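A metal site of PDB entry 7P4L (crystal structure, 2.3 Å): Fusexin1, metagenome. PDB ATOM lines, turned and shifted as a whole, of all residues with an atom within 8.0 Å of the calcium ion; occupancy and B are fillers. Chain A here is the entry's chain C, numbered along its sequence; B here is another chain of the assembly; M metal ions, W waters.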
ATOM      1  N   GLU A 341      16.190 -10.485  25.932  1.00  0.00           N
ATOM      2  CA  GLU A 341      15.100 -10.308  26.887  1.00  0.00           C
ATOM      3  C   GLU A 341      15.236 -11.275  28.058  1.00  0.00           C
ATOM      4  O   GLU A 341      15.268 -12.494  27.870  1.00  0.00           O
ATOM      5  CB  GLU A 341      13.760 -10.518  26.179  1.00  0.00           C
ATOM      6  CG  GLU A 341      12.575  -9.888  26.872  1.00  0.00           C
ATOM      7  CD  GLU A 341      11.285  -9.980  26.060  1.00  0.00           C
ATOM      8  OE1 GLU A 341      11.095 -10.993  25.341  1.00  0.00           O
ATOM      9  OE2 GLU A 341      10.462  -9.049  26.144  1.00  0.00           O
ATOM     10  N   GLY A 342      15.308 -10.732  29.276  1.00  0.00           N
ATOM     11  CA  GLY A 342      15.488 -11.498  30.485  1.00  0.00           C
ATOM     12  C   GLY A 342      16.877 -11.414  31.086  1.00  0.00           C
ATOM     13  O   GLY A 342      17.054 -11.784  32.259  1.00  0.00           O
ATOM     14  N   PHE A 397      16.329  -5.055  28.018  1.00  0.00           N
ATOM     15  CA  PHE A 397      15.409  -4.993  26.900  1.00  0.00           C
ATOM     16  C   PHE A 397      14.126  -5.739  27.230  1.00  0.00           C
ATOM     17  O   PHE A 397      14.156  -6.824  27.837  1.00  0.00           O
ATOM     18  CB  PHE A 397      16.030  -5.576  25.619  1.00  0.00           C
ATOM     19  CG  PHE A 397      15.025  -5.832  24.526  1.00  0.00           C
ATOM     20  CD1 PHE A 397      14.460  -4.784  23.824  1.00  0.00           C
ATOM     21  CD2 PHE A 397      14.637  -7.123  24.210  1.00  0.00           C
ATOM     22  CE1 PHE A 397      13.530  -5.015  22.827  1.00  0.00           C
ATOM     23  CE2 PHE A 397      13.706  -7.365  23.222  1.00  0.00           C
ATOM     24  CZ  PHE A 397      13.152  -6.310  22.520  1.00  0.00           C
ATOM     25  N   SER A 398      13.005  -5.161  26.836  1.00  0.00           N
ATOM     26  CA  SER A 398      11.703  -5.773  27.032  1.00  0.00           C
ATOM     27  C   SER A 398      10.801  -5.370  25.871  1.00  0.00           C
ATOM     28  O   SER A 398      10.953  -4.291  25.296  1.00  0.00           O
ATOM     29  CB  SER A 398      11.075  -5.349  28.363  1.00  0.00           C
ATOM     30  OG  SER A 398       9.929  -6.124  28.650  1.00  0.00           O
ATOM     31  N   SER A 399       9.882  -6.268  25.520  1.00  0.00           N
ATOM     32  CA  SER A 399       8.997  -6.058  24.393  1.00  0.00           C
ATOM     33  C   SER A 399       7.820  -7.005  24.494  1.00  0.00           C
ATOM     34  O   SER A 399       7.931  -8.090  25.073  1.00  0.00           O
ATOM     35  CB  SER A 399       9.744  -6.267  23.074  1.00  0.00           C
ATOM     36  OG  SER A 399       8.872  -6.216  21.966  1.00  0.00           O
ATOM     37  N   VAL A 400       6.681  -6.587  23.947  1.00  0.00           N
ATOM     38  CA  VAL A 400       5.499  -7.427  23.801  1.00  0.00           C
ATOM     39  C   VAL A 400       5.105  -7.594  22.347  1.00  0.00           C
ATOM     40  O   VAL A 400       4.015  -8.080  22.050  1.00  0.00           O
ATOM     41  CB  VAL A 400       4.312  -6.874  24.614  1.00  0.00           C
ATOM     42  CG1 VAL A 400       4.674  -6.775  26.078  1.00  0.00           C
ATOM     43  CG2 VAL A 400       3.873  -5.515  24.088  1.00  0.00           C
ATOM     44  N   SER A 401       5.985  -7.225  21.414  1.00  0.00           N
ATOM     45  CA  SER A 401       5.664  -7.319  20.002  1.00  0.00           C
ATOM     46  C   SER A 401       5.382  -8.762  19.616  1.00  0.00           C
ATOM     47  O   SER A 401       6.077  -9.692  20.044  1.00  0.00           O
ATOM     48  CB  SER A 401       6.808  -6.773  19.158  1.00  0.00           C
ATOM     49  OG  SER A 401       6.539  -6.983  17.781  1.00  0.00           O
ATOM     50  N   SER A 402       4.328  -8.960  18.824  1.00  0.00           N
ATOM     51  CA  SER A 402       4.028 -10.260  18.245  1.00  0.00           C
ATOM     52  C   SER A 402       4.543 -10.395  16.822  1.00  0.00           C
ATOM     53  O   SER A 402       4.366 -11.457  16.217  1.00  0.00           O
ATOM     54  CB  SER A 402       2.517 -10.493  18.268  1.00  0.00           C
ATOM     55  OG  SER A 402       1.856  -9.530  17.481  1.00  0.00           O
ATOM     56  N   SER A 404       7.891  -9.120  15.581  1.00  0.00           N
ATOM     57  CA  SER A 404       9.327  -9.138  15.391  1.00  0.00           C
ATOM     58  C   SER A 404      10.002  -9.687  16.639  1.00  0.00           C
ATOM     59  O   SER A 404       9.750  -9.195  17.742  1.00  0.00           O
ATOM     60  CB  SER A 404       9.852  -7.730  15.079  1.00  0.00           C
ATOM     61  OG  SER A 404      11.075  -7.790  14.365  1.00  0.00           O
ATOM     62  N   LYS A 405      10.853 -10.691  16.464  1.00  0.00           N
ATOM     63  CA  LYS A 405      11.646 -11.193  17.589  1.00  0.00           C
ATOM     64  C   LYS A 405      12.865 -10.314  17.852  1.00  0.00           C
ATOM     65  O   LYS A 405      13.323 -10.238  19.002  1.00  0.00           O
ATOM     66  CB  LYS A 405      12.076 -12.636  17.336  1.00  0.00           C
ATOM     67  CG  LYS A 405      12.786 -12.879  16.012  1.00  0.00           C
ATOM     68  CD  LYS A 405      12.982 -14.377  15.778  1.00  0.00           C
ATOM     69  CE  LYS A 405      13.658 -14.642  14.431  1.00  0.00           C
ATOM     70  NZ  LYS A 405      13.925 -16.084  14.226  1.00  0.00           N
ATOM     71  N   ILE A 431      16.555  -9.016  21.538  1.00  0.00           N
ATOM     72  CA  ILE A 431      15.977 -10.291  21.119  1.00  0.00           C
ATOM     73  C   ILE A 431      14.983 -10.740  22.181  1.00  0.00           C
ATOM     74  O   ILE A 431      15.329 -10.844  23.364  1.00  0.00           O
ATOM     75  CB  ILE A 431      17.058 -11.370  20.898  1.00  0.00           C
ATOM     76  CG1 ILE A 431      18.108 -10.887  19.892  1.00  0.00           C
ATOM     77  CG2 ILE A 431      16.417 -12.652  20.386  1.00  0.00           C
ATOM     78  CD1 ILE A 431      19.318 -10.254  20.525  1.00  0.00           C
ATOM     79  N   GLN A 432      13.749 -10.998  21.751  1.00  0.00           N
ATOM     80  CA  GLN A 432      12.723 -11.452  22.670  1.00  0.00           C
ATOM     81  C   GLN A 432      12.898 -12.920  23.056  1.00  0.00           C
ATOM     82  O   GLN A 432      13.498 -13.709  22.321  1.00  0.00           O
ATOM     83  CB  GLN A 432      11.340 -11.267  22.046  1.00  0.00           C
ATOM     84  CG  GLN A 432      10.936  -9.832  21.814  1.00  0.00           C
ATOM     85  CD  GLN A 432       9.439  -9.682  21.718  1.00  0.00           C
ATOM     86  OE1 GLN A 432       8.725  -9.800  22.710  1.00  0.00           O
ATOM     87  NE2 GLN A 432       8.951  -9.467  20.508  1.00  0.00           N
ATOM     88  N   GLN A 433      12.388 -13.274  24.230  1.00  0.00           N
ATOM     89  CA  GLN A 433      12.100 -14.662  24.548  1.00  0.00           C
ATOM     90  C   GLN A 433      11.010 -15.181  23.610  1.00  0.00           C
ATOM     91  O   GLN A 433      10.079 -14.447  23.261  1.00  0.00           O
ATOM     92  CB  GLN A 433      11.627 -14.815  25.993  1.00  0.00           C
ATOM     93  CG  GLN A 433      12.671 -14.510  27.053  1.00  0.00           C
ATOM     94  CD  GLN A 433      13.653 -15.652  27.255  1.00  0.00           C
ATOM     95  OE1 GLN A 433      13.350 -16.804  26.929  1.00  0.00           O
ATOM     96  NE2 GLN A 433      14.828 -15.333  27.763  1.00  0.00           N
ATOM     97  N   SER A 434      11.157 -16.426  23.178  1.00  0.00           N
ATOM     98  CA  SER A 434      10.100 -17.055  22.397  1.00  0.00           C
ATOM     99  C   SER A 434       8.906 -17.363  23.293  1.00  0.00           C
ATOM    100  O   SER A 434       9.059 -17.700  24.471  1.00  0.00           O
ATOM    101  CB  SER A 434      10.613 -18.345  21.762  1.00  0.00           C
ATOM    102  OG  SER A 434      10.987 -19.279  22.760  1.00  0.00           O
ATOM    103  N   GLU A 435       7.704 -17.190  22.741  1.00  0.00           N
ATOM    104  CA  GLU A 435       6.493 -17.589  23.433  1.00  0.00           C
ATOM    105  C   GLU A 435       6.146 -19.063  23.193  1.00  0.00           C
ATOM    106  O   GLU A 435       5.410 -19.654  23.997  1.00  0.00           O
ATOM    107  CB  GLU A 435       5.310 -16.725  22.977  1.00  0.00           C
ATOM    108  CG  GLU A 435       5.459 -15.223  23.257  1.00  0.00           C
ATOM    109  CD  GLU A 435       5.477 -14.882  24.739  1.00  0.00           C
ATOM    110  OE1 GLU A 435       4.672 -15.465  25.503  1.00  0.00           O
ATOM    111  OE2 GLU A 435       6.306 -14.036  25.132  1.00  0.00           O
ATOM    112  N   LEU A 461       6.309 -16.453  18.367  1.00  0.00           N
ATOM    113  CA  LEU A 461       5.692 -15.476  19.248  1.00  0.00           C
ATOM    114  C   LEU A 461       4.178 -15.609  19.366  1.00  0.00           C
ATOM    115  O   LEU A 461       3.622 -15.109  20.354  1.00  0.00           O
ATOM    116  CB  LEU A 461       6.016 -14.050  18.764  1.00  0.00           C
ATOM    117  CG  LEU A 461       7.493 -13.664  18.712  1.00  0.00           C
ATOM    118  CD1 LEU A 461       7.673 -12.305  18.085  1.00  0.00           C
ATOM    119  CD2 LEU A 461       8.115 -13.701  20.100  1.00  0.00           C
ATOM    120  N   TYR B 212       8.497 -13.569  32.413  1.00  0.00           N
ATOM    121  CA  TYR B 212       8.481 -12.960  31.093  1.00  0.00           C
ATOM    122  C   TYR B 212       7.453 -13.650  30.203  1.00  0.00           C
ATOM    123  O   TYR B 212       7.515 -14.872  30.005  1.00  0.00           O
ATOM    124  CB  TYR B 212       9.875 -13.031  30.461  1.00  0.00           C
ATOM    125  CG  TYR B 212      10.830 -11.989  30.984  1.00  0.00           C
ATOM    126  CD1 TYR B 212      11.598 -12.230  32.105  1.00  0.00           C
ATOM    127  CD2 TYR B 212      10.948 -10.753  30.360  1.00  0.00           C
ATOM    128  CE1 TYR B 212      12.467 -11.270  32.586  1.00  0.00           C
ATOM    129  CE2 TYR B 212      11.805  -9.800  30.829  1.00  0.00           C
ATOM    130  CZ  TYR B 212      12.560 -10.058  31.947  1.00  0.00           C
ATOM    131  OH  TYR B 212      13.431  -9.086  32.409  1.00  0.00           O
ATOM    132  N   SER B 213       6.518 -12.870  29.679  1.00  0.00           N
ATOM    133  CA  SER B 213       5.581 -13.322  28.661  1.00  0.00           C
ATOM    134  C   SER B 213       4.934 -12.105  28.021  1.00  0.00           C
ATOM    135  O   SER B 213       4.619 -11.134  28.715  1.00  0.00           O
ATOM    136  CB  SER B 213       4.494 -14.232  29.254  1.00  0.00           C
ATOM    137  OG  SER B 213       3.468 -14.495  28.312  1.00  0.00           O
ATOM    138  N   ASN B 214       4.711 -12.168  26.706  1.00  0.00           N
ATOM    139  CA  ASN B 214       4.055 -11.064  26.010  1.00  0.00           C
ATOM    140  C   ASN B 214       2.594 -10.899  26.421  1.00  0.00           C
ATOM    141  O   ASN B 214       1.971  -9.908  26.043  1.00  0.00           O
ATOM    142  CB  ASN B 214       4.143 -11.256  24.500  1.00  0.00           C
ATOM    143  CG  ASN B 214       5.559 -11.028  23.980  1.00  0.00           C
ATOM    144  OD1 ASN B 214       6.432 -10.588  24.722  1.00  0.00           O
ATOM    145  ND2 ASN B 214       5.770 -11.283  22.697  1.00  0.00           N
ATOM    146  N   ASP B 215       2.039 -11.851  27.169  1.00  0.00           N
ATOM    147  CA  ASP B 215       0.724 -11.675  27.757  1.00  0.00           C
ATOM    148  C   ASP B 215       0.713 -10.665  28.886  1.00  0.00           C
ATOM    149  O   ASP B 215      -0.362 -10.206  29.284  1.00  0.00           O
ATOM    150  CB  ASP B 215       0.185 -12.998  28.281  1.00  0.00           C
ATOM    151  CG  ASP B 215       0.038 -14.038  27.186  1.00  0.00           C
ATOM    152  OD1 ASP B 215       0.321 -13.706  26.015  1.00  0.00           O
ATOM    153  OD2 ASP B 215      -0.350 -15.183  27.506  1.00  0.00           O
ATOM    154  N   PHE B 216       1.873 -10.317  29.428  1.00  0.00           N
ATOM    155  CA  PHE B 216       1.961  -9.443  30.600  1.00  0.00           C
ATOM    156  C   PHE B 216       2.333  -8.032  30.165  1.00  0.00           C
ATOM    157  O   PHE B 216       3.022  -7.826  29.166  1.00  0.00           O
ATOM    158  CB  PHE B 216       2.994  -9.967  31.595  1.00  0.00           C
ATOM    159  CG  PHE B 216       2.779 -11.401  31.999  1.00  0.00           C
ATOM    160  CD1 PHE B 216       1.509 -11.944  32.034  1.00  0.00           C
ATOM    161  CD2 PHE B 216       3.850 -12.209  32.340  1.00  0.00           C
ATOM    162  CE1 PHE B 216       1.312 -13.274  32.402  1.00  0.00           C
ATOM    163  CE2 PHE B 216       3.663 -13.539  32.698  1.00  0.00           C
ATOM    164  CZ  PHE B 216       2.386 -14.060  32.736  1.00  0.00           C
ATOM    165  N   ASN B 218       4.111  -4.824  29.498  1.00  0.00           N
ATOM    166  CA  ASN B 218       5.518  -4.538  29.228  1.00  0.00           C
ATOM    167  C   ASN B 218       6.354  -5.800  29.008  1.00  0.00           C
ATOM    168  O   ASN B 218       7.578  -5.698  28.891  1.00  0.00           O
ATOM    169  CB  ASN B 218       6.152  -3.733  30.370  1.00  0.00           C
ATOM    170  CG  ASN B 218       5.375  -2.487  30.701  1.00  0.00           C
ATOM    171  OD1 ASN B 218       5.194  -1.618  29.849  1.00  0.00           O
ATOM    172  ND2 ASN B 218       4.890  -2.402  31.926  1.00  0.00           N
ATOM    173  N   GLY B 219       5.727  -6.960  28.927  1.00  0.00           N
ATOM    174  CA  GLY B 219       6.438  -8.176  28.610  1.00  0.00           C
ATOM    175  C   GLY B 219       6.862  -9.003  29.805  1.00  0.00           C
ATOM    176  O   GLY B 219       7.390 -10.111  29.601  1.00  0.00           O
ATOM    177  N   TRP B 220       6.670  -8.517  31.030  1.00  0.00           N
ATOM    178  CA  TRP B 220       6.973  -9.339  32.194  1.00  0.00           C
ATOM    179  C   TRP B 220       6.228  -8.820  33.424  1.00  0.00           C
ATOM    180  O   TRP B 220       5.644  -7.734  33.423  1.00  0.00           O
ATOM    181  CB  TRP B 220       8.482  -9.423  32.460  1.00  0.00           C
ATOM    182  CG  TRP B 220       9.171  -8.155  32.869  1.00  0.00           C
ATOM    183  CD1 TRP B 220       9.479  -7.102  32.071  1.00  0.00           C
ATOM    184  CD2 TRP B 220       9.670  -7.842  34.173  1.00  0.00           C
ATOM    185  NE1 TRP B 220      10.137  -6.141  32.801  1.00  0.00           N
ATOM    186  CE2 TRP B 220      10.264  -6.572  34.096  1.00  0.00           C
ATOM    187  CE3 TRP B 220       9.665  -8.507  35.404  1.00  0.00           C
ATOM    188  CZ2 TRP B 220      10.837  -5.944  35.192  1.00  0.00           C
ATOM    189  CZ3 TRP B 220      10.246  -7.891  36.498  1.00  0.00           C
ATOM    190  CH2 TRP B 220      10.821  -6.612  36.382  1.00  0.00           C
HETATM  191 CA    CA M   1       8.692 -10.317  24.960  1.00  0.00          CA
HETATM  192  O   HOH W   1       8.190 -10.785  27.078  1.00  0.00           O
HETATM  193  O   HOH W   2       8.617 -12.721  24.222  1.00  0.00           O
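Water W2 bridges the backbone carbonyl oxygen of Gln 433 (2.5 Å) and the side-chain carboxylate of Glu 435 (2.8 Å).
Of the 24 residues printed, 4 come within 4 Å of the calcium ion.
The nearest printed residue that does not touch the calcium ion is Val 400 (4.4 Å).
Water W1 binds the calcium ion, at 2.2 Å.
OD1 of Asn 214 of chain B is bound to the calcium ion (2.3 Å).
The side-chain amide oxygen (OE1) of Gln 432 is bound to the calcium ion.
The calcium ion is bound by O of Ser 399, 2.4 Å away.
The calcium ion is bound by OE2 of Glu 341 (2.5 Å).
Water W2 is bound to the calcium ion.
The calcium ion is bound by OE1 of Glu 341, 2.5 Å away.
The backbone NH (N) of Gln 432 is in hydrogen-bond range of the backbone carbonyl oxygen (O) of Lys 405 (2.9 Å).
O of Ile 431 is in hydrogen-bond range of N of Glu 341, at 2.7 Å.
The side-chain hydroxyl of Ser 399 sits at hydrogen-bond distance from the backbone NH of Ser 401 (3.1 Å).
O of Ser 401 lies within hydrogen-bond range of NE2 of Gln 432 (2.9 Å).
N of Asn 214 of chain B sits at hydrogen-bond distance from OE2 of Glu 435 (2.9 Å).
NE2 of Gln 432 lies within hydrogen-bond range of O of Ser 404, at 2.9 Å.
O of Ser 401 sits at hydrogen-bond distance from ND2 of Asn 214 of chain B, at 3.1 Å.
The side-chain amide nitrogen of Gln 433 sits at hydrogen-bond distance from the backbone carbonyl oxygen of Glu 341 (2.9 Å).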
